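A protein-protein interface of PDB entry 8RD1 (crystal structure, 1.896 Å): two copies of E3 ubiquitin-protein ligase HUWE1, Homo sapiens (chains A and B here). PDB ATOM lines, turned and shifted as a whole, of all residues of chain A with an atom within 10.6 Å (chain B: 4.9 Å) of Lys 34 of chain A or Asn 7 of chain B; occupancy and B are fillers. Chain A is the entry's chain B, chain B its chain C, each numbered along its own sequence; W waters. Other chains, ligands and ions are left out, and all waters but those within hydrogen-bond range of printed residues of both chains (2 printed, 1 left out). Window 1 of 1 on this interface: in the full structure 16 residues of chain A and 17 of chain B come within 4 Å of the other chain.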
ATOM      1  N   ASN A   6      10.141  -7.255  12.431  1.00  0.00           N
ATOM      2  CA  ASN A   6      11.571  -7.069  12.191  1.00  0.00           C
ATOM      3  C   ASN A   6      11.902  -5.740  11.426  1.00  0.00           C
ATOM      4  O   ASN A   6      12.278  -4.775  12.094  1.00  0.00           O
ATOM      5  CB  ASN A   6      12.183  -8.316  11.511  1.00  0.00           C
ATOM      6  CG  ASN A   6      13.629  -8.154  11.070  1.00  0.00           C
ATOM      7  OD1 ASN A   6      14.455  -7.510  11.747  1.00  0.00           O
ATOM      8  ND2 ASN A   6      13.975  -8.726   9.915  1.00  0.00           N
ATOM      9  N   ASN A   7      11.792  -5.678  10.077  1.00  0.00           N
ATOM     10  CA  ASN A   7      12.253  -4.505   9.342  1.00  0.00           C
ATOM     11  C   ASN A   7      11.166  -3.484   8.967  1.00  0.00           C
ATOM     12  O   ASN A   7      11.526  -2.335   8.745  1.00  0.00           O
ATOM     13  CB  ASN A   7      13.066  -4.898   8.098  1.00  0.00           C
ATOM     14  CG  ASN A   7      12.387  -5.806   7.088  1.00  0.00           C
ATOM     15  OD1 ASN A   7      11.545  -6.649   7.420  1.00  0.00           O
ATOM     16  ND2 ASN A   7      12.790  -5.698   5.827  1.00  0.00           N
ATOM     17  N   TRP A   8       9.873  -3.861   8.918  1.00  0.00           N
ATOM     18  CA  TRP A   8       8.809  -2.898   8.615  1.00  0.00           C
ATOM     19  C   TRP A   8       8.269  -2.296   9.892  1.00  0.00           C
ATOM     20  O   TRP A   8       8.260  -2.952  10.930  1.00  0.00           O
ATOM     21  CB  TRP A   8       7.670  -3.563   7.830  1.00  0.00           C
ATOM     22  CG  TRP A   8       8.034  -3.820   6.404  1.00  0.00           C
ATOM     23  CD1 TRP A   8       8.776  -4.860   5.925  1.00  0.00           C
ATOM     24  CD2 TRP A   8       7.863  -2.914   5.315  1.00  0.00           C
ATOM     25  NE1 TRP A   8       8.981  -4.706   4.576  1.00  0.00           N
ATOM     26  CE2 TRP A   8       8.427  -3.520   4.175  1.00  0.00           C
ATOM     27  CE3 TRP A   8       7.224  -1.672   5.172  1.00  0.00           C
ATOM     28  CZ2 TRP A   8       8.374  -2.931   2.923  1.00  0.00           C
ATOM     29  CZ3 TRP A   8       7.193  -1.085   3.929  1.00  0.00           C
ATOM     30  CH2 TRP A   8       7.804  -1.690   2.831  1.00  0.00           C
ATOM     31  N   ASN A  26       5.136  -9.079   9.416  1.00  0.00           N
ATOM     32  CA  ASN A  26       6.344  -8.524   8.821  1.00  0.00           C
ATOM     33  C   ASN A  26       6.783  -9.366   7.621  1.00  0.00           C
ATOM     34  O   ASN A  26       7.095  -8.808   6.575  1.00  0.00           O
ATOM     35  CB  ASN A  26       7.479  -8.455   9.837  1.00  0.00           C
ATOM     36  CG  ASN A  26       8.649  -7.705   9.294  1.00  0.00           C
ATOM     37  OD1 ASN A  26       8.646  -6.485   9.271  1.00  0.00           O
ATOM     38  ND2 ASN A  26       9.671  -8.413   8.817  1.00  0.00           N
ATOM     39  N   SER A  27       6.738 -10.709   7.764  1.00  0.00           N
ATOM     40  CA  SER A  27       7.080 -11.624   6.681  1.00  0.00           C
ATOM     41  C   SER A  27       6.114 -11.466   5.497  1.00  0.00           C
ATOM     42  O   SER A  27       6.573 -11.404   4.364  1.00  0.00           O
ATOM     43  CB  SER A  27       7.080 -13.066   7.184  1.00  0.00           C
ATOM     44  OG  SER A  27       7.388 -13.952   6.126  1.00  0.00           O
ATOM     45  N   THR A  28       4.793 -11.363   5.754  1.00  0.00           N
ATOM     46  CA  THR A  28       3.818 -11.153   4.685  1.00  0.00           C
ATOM     47  C   THR A  28       4.091  -9.857   3.920  1.00  0.00           C
ATOM     48  O   THR A  28       4.052  -9.843   2.683  1.00  0.00           O
ATOM     49  CB  THR A  28       2.394 -11.139   5.253  1.00  0.00           C
ATOM     50  OG1 THR A  28       2.097 -12.410   5.829  1.00  0.00           O
ATOM     51  CG2 THR A  28       1.347 -10.800   4.202  1.00  0.00           C
ATOM     52  N   ILE A  29       4.367  -8.765   4.650  1.00  0.00           N
ATOM     53  CA  ILE A  29       4.616  -7.476   4.020  1.00  0.00           C
ATOM     54  C   ILE A  29       5.924  -7.527   3.236  1.00  0.00           C
ATOM     55  O   ILE A  29       5.954  -7.118   2.083  1.00  0.00           O
ATOM     56  CB  ILE A  29       4.624  -6.332   5.078  1.00  0.00           C
ATOM     57  CG1 ILE A  29       3.214  -6.162   5.726  1.00  0.00           C
ATOM     58  CG2 ILE A  29       5.125  -5.002   4.470  1.00  0.00           C
ATOM     59  CD1 ILE A  29       3.223  -5.467   7.048  1.00  0.00           C
ATOM     60  N   ASP A  30       6.995  -8.038   3.856  1.00  0.00           N
ATOM     61  CA  ASP A  30       8.304  -8.085   3.209  1.00  0.00           C
ATOM     62  C   ASP A  30       8.326  -9.010   1.980  1.00  0.00           C
ATOM     63  O   ASP A  30       8.974  -8.661   1.001  1.00  0.00           O
ATOM     64  CB  ASP A  30       9.401  -8.459   4.224  1.00  0.00           C
ATOM     65  CG  ASP A  30      10.777  -7.986   3.829  1.00  0.00           C
ATOM     66  OD1 ASP A  30      10.939  -6.768   3.565  1.00  0.00           O
ATOM     67  OD2 ASP A  30      11.691  -8.826   3.766  1.00  0.00           O
ATOM     68  N   SER A  31       7.569 -10.123   1.982  1.00  0.00           N
ATOM     69  CA  SER A  31       7.507 -11.000   0.799  1.00  0.00           C
ATOM     70  C   SER A  31       6.845 -10.269  -0.356  1.00  0.00           C
ATOM     71  O   SER A  31       7.328 -10.340  -1.489  1.00  0.00           O
ATOM     72  CB  SER A  31       6.726 -12.281   1.092  1.00  0.00           C
ATOM     73  OG  SER A  31       7.399 -13.057   2.066  1.00  0.00           O
ATOM     74  N   ALA A  32       5.752  -9.538  -0.080  1.00  0.00           N
ATOM     75  CA  ALA A  32       5.068  -8.781  -1.130  1.00  0.00           C
ATOM     76  C   ALA A  32       5.954  -7.629  -1.627  1.00  0.00           C
ATOM     77  O   ALA A  32       5.989  -7.343  -2.833  1.00  0.00           O
ATOM     78  CB  ALA A  32       3.754  -8.254  -0.612  1.00  0.00           C
ATOM     79  N   TRP A  33       6.685  -6.983  -0.712  1.00  0.00           N
ATOM     80  CA  TRP A  33       7.616  -5.924  -1.083  1.00  0.00           C
ATOM     81  C   TRP A  33       8.690  -6.472  -2.077  1.00  0.00           C
ATOM     82  O   TRP A  33       8.887  -5.908  -3.148  1.00  0.00           O
ATOM     83  CB  TRP A  33       8.321  -5.376   0.166  1.00  0.00           C
ATOM     84  CG  TRP A  33       9.390  -4.377  -0.148  1.00  0.00           C
ATOM     85  CD1 TRP A  33      10.741  -4.568  -0.083  1.00  0.00           C
ATOM     86  CD2 TRP A  33       9.193  -3.057  -0.658  1.00  0.00           C
ATOM     87  NE1 TRP A  33      11.397  -3.428  -0.493  1.00  0.00           N
ATOM     88  CE2 TRP A  33      10.470  -2.488  -0.860  1.00  0.00           C
ATOM     89  CE3 TRP A  33       8.058  -2.276  -0.917  1.00  0.00           C
ATOM     90  CZ2 TRP A  33      10.639  -1.181  -1.303  1.00  0.00           C
ATOM     91  CZ3 TRP A  33       8.234  -0.983  -1.367  1.00  0.00           C
ATOM     92  CH2 TRP A  33       9.508  -0.438  -1.513  1.00  0.00           C
ATOM     93  N   LYS A  34       9.331  -7.590  -1.724  1.00  0.00           N
ATOM     94  CA  LYS A  34      10.380  -8.169  -2.563  1.00  0.00           C
ATOM     95  C   LYS A  34       9.839  -8.691  -3.906  1.00  0.00           C
ATOM     96  O   LYS A  34      10.596  -8.721  -4.876  1.00  0.00           O
ATOM     97  CB  LYS A  34      11.120  -9.278  -1.807  1.00  0.00           C
ATOM     98  CG  LYS A  34      11.984  -8.785  -0.643  1.00  0.00           C
ATOM     99  CD  LYS A  34      12.579  -9.969   0.172  1.00  0.00           C
ATOM    100  CE  LYS A  34      13.997  -9.761   0.666  1.00  0.00           C
ATOM    101  NZ  LYS A  34      14.150  -8.559   1.550  1.00  0.00           N
ATOM    102  N   SER A  35       8.548  -9.080  -3.978  1.00  0.00           N
ATOM    103  CA  SER A  35       7.951  -9.584  -5.224  1.00  0.00           C
ATOM    104  C   SER A  35       7.470  -8.494  -6.188  1.00  0.00           C
ATOM    105  O   SER A  35       6.905  -8.825  -7.222  1.00  0.00           O
ATOM    106  CB  SER A  35       6.788 -10.510  -4.900  1.00  0.00           C
ATOM    107  OG  SER A  35       5.764  -9.759  -4.274  1.00  0.00           O
ATOM    108  N   GLY A  36       7.648  -7.220  -5.849  1.00  0.00           N
ATOM    109  CA  GLY A  36       7.261  -6.126  -6.728  1.00  0.00           C
ATOM    110  C   GLY A  36       5.805  -5.715  -6.678  1.00  0.00           C
ATOM    111  O   GLY A  36       5.408  -4.843  -7.449  1.00  0.00           O
ATOM    112  N   GLU A  37       4.999  -6.296  -5.769  1.00  0.00           N
ATOM    113  CA  GLU A  37       3.580  -5.927  -5.660  1.00  0.00           C
ATOM    114  C   GLU A  37       3.428  -4.455  -5.240  1.00  0.00           C
ATOM    115  O   GLU A  37       4.265  -3.968  -4.501  1.00  0.00           O
ATOM    116  CB  GLU A  37       2.876  -6.802  -4.615  1.00  0.00           C
ATOM    117  CG  GLU A  37       2.739  -8.259  -5.012  1.00  0.00           C
ATOM    118  CD  GLU A  37       2.142  -9.112  -3.919  1.00  0.00           C
ATOM    119  OE1 GLU A  37       1.351  -8.571  -3.113  1.00  0.00           O
ATOM    120  OE2 GLU A  37       2.451 -10.324  -3.871  1.00  0.00           O
ATOM    121  N   THR A  38       2.356  -3.776  -5.672  1.00  0.00           N
ATOM    122  CA  THR A  38       2.117  -2.388  -5.312  1.00  0.00           C
ATOM    123  C   THR A  38       1.402  -2.249  -3.941  1.00  0.00           C
ATOM    124  O   THR A  38       1.414  -1.160  -3.383  1.00  0.00           O
ATOM    125  CB  THR A  38       1.331  -1.672  -6.403  1.00  0.00           C
ATOM    126  OG1 THR A  38       0.123  -2.387  -6.631  1.00  0.00           O
ATOM    127  CG2 THR A  38       2.142  -1.527  -7.723  1.00  0.00           C
ATOM    128  N   SER A  39       0.804  -3.328  -3.421  1.00  0.00           N
ATOM    129  CA  SER A  39       0.096  -3.344  -2.136  1.00  0.00           C
ATOM    130  C   SER A  39       0.027  -4.785  -1.594  1.00  0.00           C
ATOM    131  O   SER A  39       0.283  -5.750  -2.338  1.00  0.00           O
ATOM    132  CB  SER A  39      -1.318  -2.783  -2.298  1.00  0.00           C
ATOM    133  OG  SER A  39      -2.108  -3.637  -3.108  1.00  0.00           O
ATOM    134  N   VAL A  40      -0.282  -4.932  -0.302  1.00  0.00           N
ATOM    135  CA  VAL A  40      -0.380  -6.240   0.341  1.00  0.00           C
ATOM    136  C   VAL A  40      -1.424  -6.176   1.445  1.00  0.00           C
ATOM    137  O   VAL A  40      -1.506  -5.171   2.165  1.00  0.00           O
ATOM    138  CB  VAL A  40       0.982  -6.736   0.881  1.00  0.00           C
ATOM    139  CG1 VAL A  40       1.601  -5.745   1.877  1.00  0.00           C
ATOM    140  CG2 VAL A  40       0.877  -8.143   1.486  1.00  0.00           C
ATOM    141  N   PHE A  53       2.194   0.293  -0.946  1.00  0.00           N
ATOM    142  CA  PHE A  53       3.606   0.617  -1.167  1.00  0.00           C
ATOM    143  C   PHE A  53       3.855   1.859  -2.026  1.00  0.00           C
ATOM    144  O   PHE A  53       4.947   2.444  -1.942  1.00  0.00           O
ATOM    145  CB  PHE A  53       4.330  -0.591  -1.761  1.00  0.00           C
ATOM    146  CG  PHE A  53       4.376  -1.827  -0.884  1.00  0.00           C
ATOM    147  CD1 PHE A  53       4.817  -1.755   0.428  1.00  0.00           C
ATOM    148  CD2 PHE A  53       4.065  -3.077  -1.403  1.00  0.00           C
ATOM    149  CE1 PHE A  53       4.897  -2.889   1.206  1.00  0.00           C
ATOM    150  CE2 PHE A  53       4.217  -4.219  -0.639  1.00  0.00           C
ATOM    151  CZ  PHE A  53       4.616  -4.123   0.658  1.00  0.00           C
ATOM    152  N   LEU A  71      10.329   1.288   6.009  1.00  0.00           N
ATOM    153  CA  LEU A  71      11.176   0.122   5.873  1.00  0.00           C
ATOM    154  C   LEU A  71      12.537   0.496   6.472  1.00  0.00           C
ATOM    155  O   LEU A  71      13.133   1.456   6.020  1.00  0.00           O
ATOM    156  CB  LEU A  71      11.310  -0.207   4.362  1.00  0.00           C
ATOM    157  CG  LEU A  71      12.268  -1.319   3.967  1.00  0.00           C
ATOM    158  CD1 LEU A  71      11.937  -2.624   4.676  1.00  0.00           C
ATOM    159  CD2 LEU A  71      12.204  -1.547   2.479  1.00  0.00           C
ATOM    160  N   THR A  72      13.001  -0.221   7.496  1.00  0.00           N
ATOM    161  CA  THR A  72      14.315  -0.014   8.101  1.00  0.00           C
ATOM    162  C   THR A  72      15.386  -0.348   7.049  1.00  0.00           C
ATOM    163  O   THR A  72      15.197  -1.284   6.268  1.00  0.00           O
ATOM    164  CB  THR A  72      14.484  -0.937   9.341  1.00  0.00           C
ATOM    165  OG1 THR A  72      13.606  -0.509  10.365  1.00  0.00           O
ATOM    166  CG2 THR A  72      15.896  -0.943   9.919  1.00  0.00           C
ATOM    167  N   LEU A  73      16.461   0.437   6.991  1.00  0.00           N
ATOM    168  CA  LEU A  73      17.566   0.217   6.050  1.00  0.00           C
ATOM    169  C   LEU A  73      18.820   0.034   6.886  1.00  0.00           C
ATOM    170  O   LEU A  73      19.147   0.896   7.706  1.00  0.00           O
ATOM    171  CB  LEU A  73      17.707   1.406   5.096  1.00  0.00           C
ATOM    172  CG  LEU A  73      18.774   1.364   3.954  1.00  0.00           C
ATOM    173  CD1 LEU A  73      18.305   0.531   2.752  1.00  0.00           C
ATOM    174  CD2 LEU A  73      19.078   2.791   3.454  1.00  0.00           C
ATOM    175  N   LEU A  74      19.505  -1.103   6.703  1.00  0.00           N
ATOM    176  CA  LEU A  74      20.713  -1.394   7.447  1.00  0.00           C
ATOM    177  C   LEU A  74      21.921  -0.841   6.702  1.00  0.00           C
ATOM    178  O   LEU A  74      21.905  -0.722   5.476  1.00  0.00           O
ATOM    179  CB  LEU A  74      20.841  -2.905   7.749  1.00  0.00           C
ATOM    180  CG  LEU A  74      19.618  -3.551   8.459  1.00  0.00           C
ATOM    181  CD1 LEU A  74      19.749  -5.057   8.498  1.00  0.00           C
ATOM    182  CD2 LEU A  74      19.403  -2.997   9.887  1.00  0.00           C
ATOM    183  N   VAL A  76      25.405  -0.200   4.889  1.00  0.00           N
ATOM    184  CA  VAL A  76      26.182  -0.938   3.902  1.00  0.00           C
ATOM    185  C   VAL A  76      27.489  -0.165   3.690  1.00  0.00           C
ATOM    186  O   VAL A  76      27.416   0.987   3.250  1.00  0.00           O
ATOM    187  CB  VAL A  76      25.458  -1.135   2.551  1.00  0.00           C
ATOM    188  CG1 VAL A  76      26.398  -1.772   1.523  1.00  0.00           C
ATOM    189  CG2 VAL A  76      24.199  -1.989   2.721  1.00  0.00           C
ATOM    190  N   ASN B   6      15.606 -12.813  -5.071  1.00  0.00           N
ATOM    191  CA  ASN B   6      17.031 -12.874  -5.369  1.00  0.00           C
ATOM    192  C   ASN B   6      17.623 -11.460  -5.400  1.00  0.00           C
ATOM    193  O   ASN B   6      17.945 -10.923  -6.456  1.00  0.00           O
ATOM    194  CB  ASN B   6      17.282 -13.668  -6.659  1.00  0.00           C
ATOM    195  CG  ASN B   6      17.336 -15.174  -6.432  1.00  0.00           C
ATOM    196  OD1 ASN B   6      18.314 -15.842  -6.794  1.00  0.00           O
ATOM    197  ND2 ASN B   6      16.300 -15.748  -5.809  1.00  0.00           N
ATOM    198  N   ASN B   7      17.808 -10.886  -4.195  1.00  0.00           N
ATOM    199  CA  ASN B   7      18.315  -9.525  -4.008  1.00  0.00           C
ATOM    200  C   ASN B   7      19.855  -9.393  -3.870  1.00  0.00           C
ATOM    201  O   ASN B   7      20.362  -8.296  -4.085  1.00  0.00           O
ATOM    202  CB  ASN B   7      17.623  -8.838  -2.827  1.00  0.00           C
ATOM    203  CG  ASN B   7      17.705  -9.554  -1.488  1.00  0.00           C
ATOM    204  OD1 ASN B   7      17.731 -10.793  -1.407  1.00  0.00           O
ATOM    205  ND2 ASN B   7      17.678  -8.788  -0.397  1.00  0.00           N
ATOM    206  N   TRP B   8      20.591 -10.463  -3.509  1.00  0.00           N
ATOM    207  CA  TRP B   8      22.062 -10.376  -3.431  1.00  0.00           C
ATOM    208  C   TRP B   8      22.679 -10.719  -4.786  1.00  0.00           C
ATOM    209  O   TRP B   8      22.108 -11.490  -5.548  1.00  0.00           O
ATOM    210  CB  TRP B   8      22.608 -11.307  -2.341  1.00  0.00           C
ATOM    211  CG  TRP B   8      22.341 -10.798  -0.959  1.00  0.00           C
ATOM    212  CD1 TRP B   8      21.173 -10.901  -0.263  1.00  0.00           C
ATOM    213  CD2 TRP B   8      23.202  -9.965  -0.181  1.00  0.00           C
ATOM    214  NE1 TRP B   8      21.272 -10.222   0.927  1.00  0.00           N
ATOM    215  CE2 TRP B   8      22.503  -9.623   0.995  1.00  0.00           C
ATOM    216  CE3 TRP B   8      24.490  -9.448  -0.379  1.00  0.00           C
ATOM    217  CZ2 TRP B   8      23.053  -8.805   1.975  1.00  0.00           C
ATOM    218  CZ3 TRP B   8      25.045  -8.654   0.601  1.00  0.00           C
ATOM    219  CH2 TRP B   8      24.326  -8.322   1.755  1.00  0.00           C
ATOM    220  N   ARG B   9      23.832 -10.119  -5.105  1.00  0.00           N
ATOM    221  CA  ARG B   9      24.537 -10.422  -6.347  1.00  0.00           C
ATOM    222  C   ARG B   9      26.048 -10.465  -6.084  1.00  0.00           C
ATOM    223  O   ARG B   9      26.538  -9.793  -5.182  1.00  0.00           O
ATOM    224  CB  ARG B   9      24.265  -9.383  -7.443  1.00  0.00           C
ATOM    225  CG  ARG B   9      22.787  -9.030  -7.693  1.00  0.00           C
ATOM    226  CD  ARG B   9      22.293  -9.458  -9.053  1.00  0.00           C
ATOM    227  NE  ARG B   9      20.951  -8.968  -9.361  1.00  0.00           N
ATOM    228  CZ  ARG B   9      19.803  -9.491  -8.935  1.00  0.00           C
ATOM    229  NH1 ARG B   9      18.644  -8.944  -9.293  1.00  0.00           N
ATOM    230  NH2 ARG B   9      19.802 -10.554  -8.128  1.00  0.00           N
ATOM    231  N   ASN B  26      20.745 -17.323  -1.615  1.00  0.00           N
ATOM    232  CA  ASN B  26      20.267 -15.959  -1.404  1.00  0.00           C
ATOM    233  C   ASN B  26      19.527 -15.860  -0.065  1.00  0.00           C
ATOM    234  O   ASN B  26      19.771 -14.934   0.690  1.00  0.00           O
ATOM    235  CB  ASN B  26      19.349 -15.514  -2.542  1.00  0.00           C
ATOM    236  CG  ASN B  26      19.020 -14.055  -2.433  1.00  0.00           C
ATOM    237  OD1 ASN B  26      19.828 -13.200  -2.801  1.00  0.00           O
ATOM    238  ND2 ASN B  26      17.861 -13.727  -1.863  1.00  0.00           N
ATOM    239  N   ASP B  30      20.645 -13.540   2.990  1.00  0.00           N
ATOM    240  CA  ASP B  30      19.701 -12.526   3.447  1.00  0.00           C
ATOM    241  C   ASP B  30      19.231 -12.739   4.906  1.00  0.00           C
ATOM    242  O   ASP B  30      19.098 -11.757   5.630  1.00  0.00           O
ATOM    243  CB  ASP B  30      18.521 -12.425   2.475  1.00  0.00           C
ATOM    244  CG  ASP B  30      17.867 -11.065   2.477  1.00  0.00           C
ATOM    245  OD1 ASP B  30      18.597 -10.051   2.299  1.00  0.00           O
ATOM    246  OD2 ASP B  30      16.635 -11.007   2.665  1.00  0.00           O
ATOM    247  N   LYS B  34      19.875  -9.913   7.804  1.00  0.00           N
ATOM    248  CA  LYS B  34      18.807  -9.375   8.655  1.00  0.00           C
ATOM    249  C   LYS B  34      19.024  -9.654  10.148  1.00  0.00           C
ATOM    250  O   LYS B  34      18.538  -8.884  10.980  1.00  0.00           O
ATOM    251  CB  LYS B  34      17.454  -9.908   8.191  1.00  0.00           C
ATOM    252  CG  LYS B  34      17.016  -9.373   6.832  1.00  0.00           C
ATOM    253  CD  LYS B  34      15.725 -10.026   6.392  1.00  0.00           C
ATOM    254  CE  LYS B  34      15.166  -9.365   5.167  1.00  0.00           C
ATOM    255  NZ  LYS B  34      13.905 -10.007   4.702  1.00  0.00           N
ATOM    256  N   MET B  70      26.970  -7.264  -3.858  1.00  0.00           N
ATOM    257  CA  MET B  70      26.079  -6.135  -3.687  1.00  0.00           C
ATOM    258  C   MET B  70      24.689  -6.593  -3.260  1.00  0.00           C
ATOM    259  O   MET B  70      24.279  -7.715  -3.510  1.00  0.00           O
ATOM    260  CB  MET B  70      26.032  -5.243  -4.935  1.00  0.00           C
ATOM    261  CG  MET B  70      25.274  -5.806  -6.109  1.00  0.00           C
ATOM    262  SD  MET B  70      24.878  -4.554  -7.369  1.00  0.00           S
ATOM    263  CE  MET B  70      23.568  -3.750  -6.660  1.00  0.00           C
ATOM    264  N   LEU B  71      23.973  -5.691  -2.615  1.00  0.00           N
ATOM    265  CA  LEU B  71      22.603  -5.902  -2.192  1.00  0.00           C
ATOM    266  C   LEU B  71      21.757  -4.956  -3.035  1.00  0.00           C
ATOM    267  O   LEU B  71      22.013  -3.764  -3.011  1.00  0.00           O
ATOM    268  CB  LEU B  71      22.502  -5.532  -0.704  1.00  0.00           C
ATOM    269  CG  LEU B  71      21.117  -5.524  -0.061  1.00  0.00           C
ATOM    270  CD1 LEU B  71      20.431  -6.873  -0.203  1.00  0.00           C
ATOM    271  CD2 LEU B  71      21.257  -5.216   1.419  1.00  0.00           C
ATOM    272  N   THR B  72      20.801  -5.473  -3.788  1.00  0.00           N
ATOM    273  CA  THR B  72      19.948  -4.641  -4.627  1.00  0.00           C
ATOM    274  C   THR B  72      18.974  -3.916  -3.700  1.00  0.00           C
ATOM    275  O   THR B  72      18.625  -4.424  -2.627  1.00  0.00           O
ATOM    276  CB  THR B  72      19.240  -5.450  -5.731  1.00  0.00           C
ATOM    277  OG1 THR B  72      18.382  -6.397  -5.141  1.00  0.00           O
ATOM    278  CG2 THR B  72      20.195  -6.167  -6.639  1.00  0.00           C
ATOM    279  N   LEU B  74      15.311  -1.685  -3.596  1.00  0.00           N
ATOM    280  CA  LEU B  74      14.110  -1.299  -4.312  1.00  0.00           C
ATOM    281  C   LEU B  74      13.701   0.127  -3.922  1.00  0.00           C
ATOM    282  O   LEU B  74      13.967   0.578  -2.813  1.00  0.00           O
ATOM    283  CB  LEU B  74      12.985  -2.318  -4.096  1.00  0.00           C
ATOM    284  CG  LEU B  74      13.362  -3.794  -4.463  1.00  0.00           C
ATOM    285  CD1 LEU B  74      12.313  -4.762  -4.036  1.00  0.00           C
ATOM    286  CD2 LEU B  74      13.650  -3.973  -5.987  1.00  0.00           C
HETATM  287  O   HOH W   1      14.646  -3.400  -0.915  1.00  0.00           O
HETATM  288  O   HOH W   2      17.333  -7.788   2.506  1.00  0.00           O
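OD2 of Asp 30 of chain A lies within salt-bridge range of NZ of Lys 34 of chain B (2.7 Å). OD2 of Asp 30 of chain B is in salt-bridge range of NZ of Lys 34 of chain A. NZ of Lys 34 of chain A sits close to NZ of Lys 34 of chain B (3.5 Å).
OD1 of Asp 30 of chain A is in hydrogen-bond range of NE1 of Trp 8 of chain A (3.0 Å). The side-chain carboxylate of Asp 30 of chain A lies within salt-bridge range of the side-chain amino group of Lys 34 of chain A, 3.3 Å away. ND2 of Asn 26 of chain B lies within hydrogen-bond range of OD1 of Asn 7 of chain B (3.0 Å). O of Asn 7 of chain B lies within hydrogen-bond range of N of Thr 72 of chain B, 2.9 Å away. The side-chain carboxylate of Asp 30 of chain B lies within hydrogen-bond range of the indole nitrogen of Trp 8 of chain B (3.0 Å). The side-chain amino group of Lys 34 of chain B is in salt-bridge range of the side-chain carboxylate of Asp 30 of chain B.
Leu 74 of chain B touches Trp 33 of chain A (CD1 to O, 3.7 Å). Asn 7 of chain B touches Lys 34 of chain A (ND2 to CE, 3.95 Å).
Ser 27 of chain A touches none of the printed residues of chain B. Of the printed residues of chain B, Asp 30 of chain A touches Lys 34 (2.7 Å). Ser 31 of chain A touches none of the printed residues of chain B. Of the printed residues of chain B, Trp 33 of chain A touches Leu 74 (3.7 Å). Of chain A, only Lys 34 (3.95 Å) comes within 4 Å of Asn 7 of chain B. No residue of chain A comes within 4 Å of Arg 9 of chain B. Printed residues of chain A within 4 Å of Asp 30 of chain B: Lys 34 (3.5 Å). Printed residues of chain A within 4 Å of Lys 34 of chain B: Asp 30 (2.7 Å) and Lys 34 (3.5 Å). No residue of chain A comes within 4 Å of Leu 71 of chain B. No residue of chain A comes within 4 Å of Thr 72 of chain B. The nearest residue of chain A that does not touch Asn 7 of chain B is Asp 30 of chain A (7.3 Å). The nearest printed residue of chain A that does not touch Lys 34 of chain B is Asn 6 of chain A (4.1 Å).
Of the 24 printed residues of chain A, 3 touch a printed residue of chain B. Hydrophobic or aromatic side chains of chain A that line the printed part of chain B: Trp 33. Hydrophobic or aromatic side chains of chain B within 4 Å of the printed part of chain A: Leu 74. Among the printed residues, 5 pairs touch across the chains. Among the printed residues, Asp or Glu carboxylates within 4 Å of a Lys or Arg side-chain nitrogen of the other chain: Asp 30 of chain A with Lys 34 of chain B (2.7 Å) and Lys 34 of chain A with Asp 30 of chain B (3.7 Å).
Asp 30 of chain A touches Lys 34 of chain B, and with the chains exchanged Lys 34 of chain A touches Asp 30 of chain B. Lys 34 of chain A touches Asn 7 of chain B, but with the chains exchanged Asn 7 of chain A does not touch Lys 34 of chain B (4.4 Å). Lys 34 of chain B touches its own counterpart, Lys 34 of chain A.
Water W2 lies within hydrogen-bond range of OD1 of Asp 30 of chain B (2.6 Å), ND2 of Asn 7 of chain B (3.1 Å) and NZ of Lys 34 of chain A (3.4 Å). Water W1 bridges the backbone NH (N) of Leu 74 of chain B (3.3 Å) and the indole nitrogen (NE1) of Trp 33 of chain A (3.3 Å).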
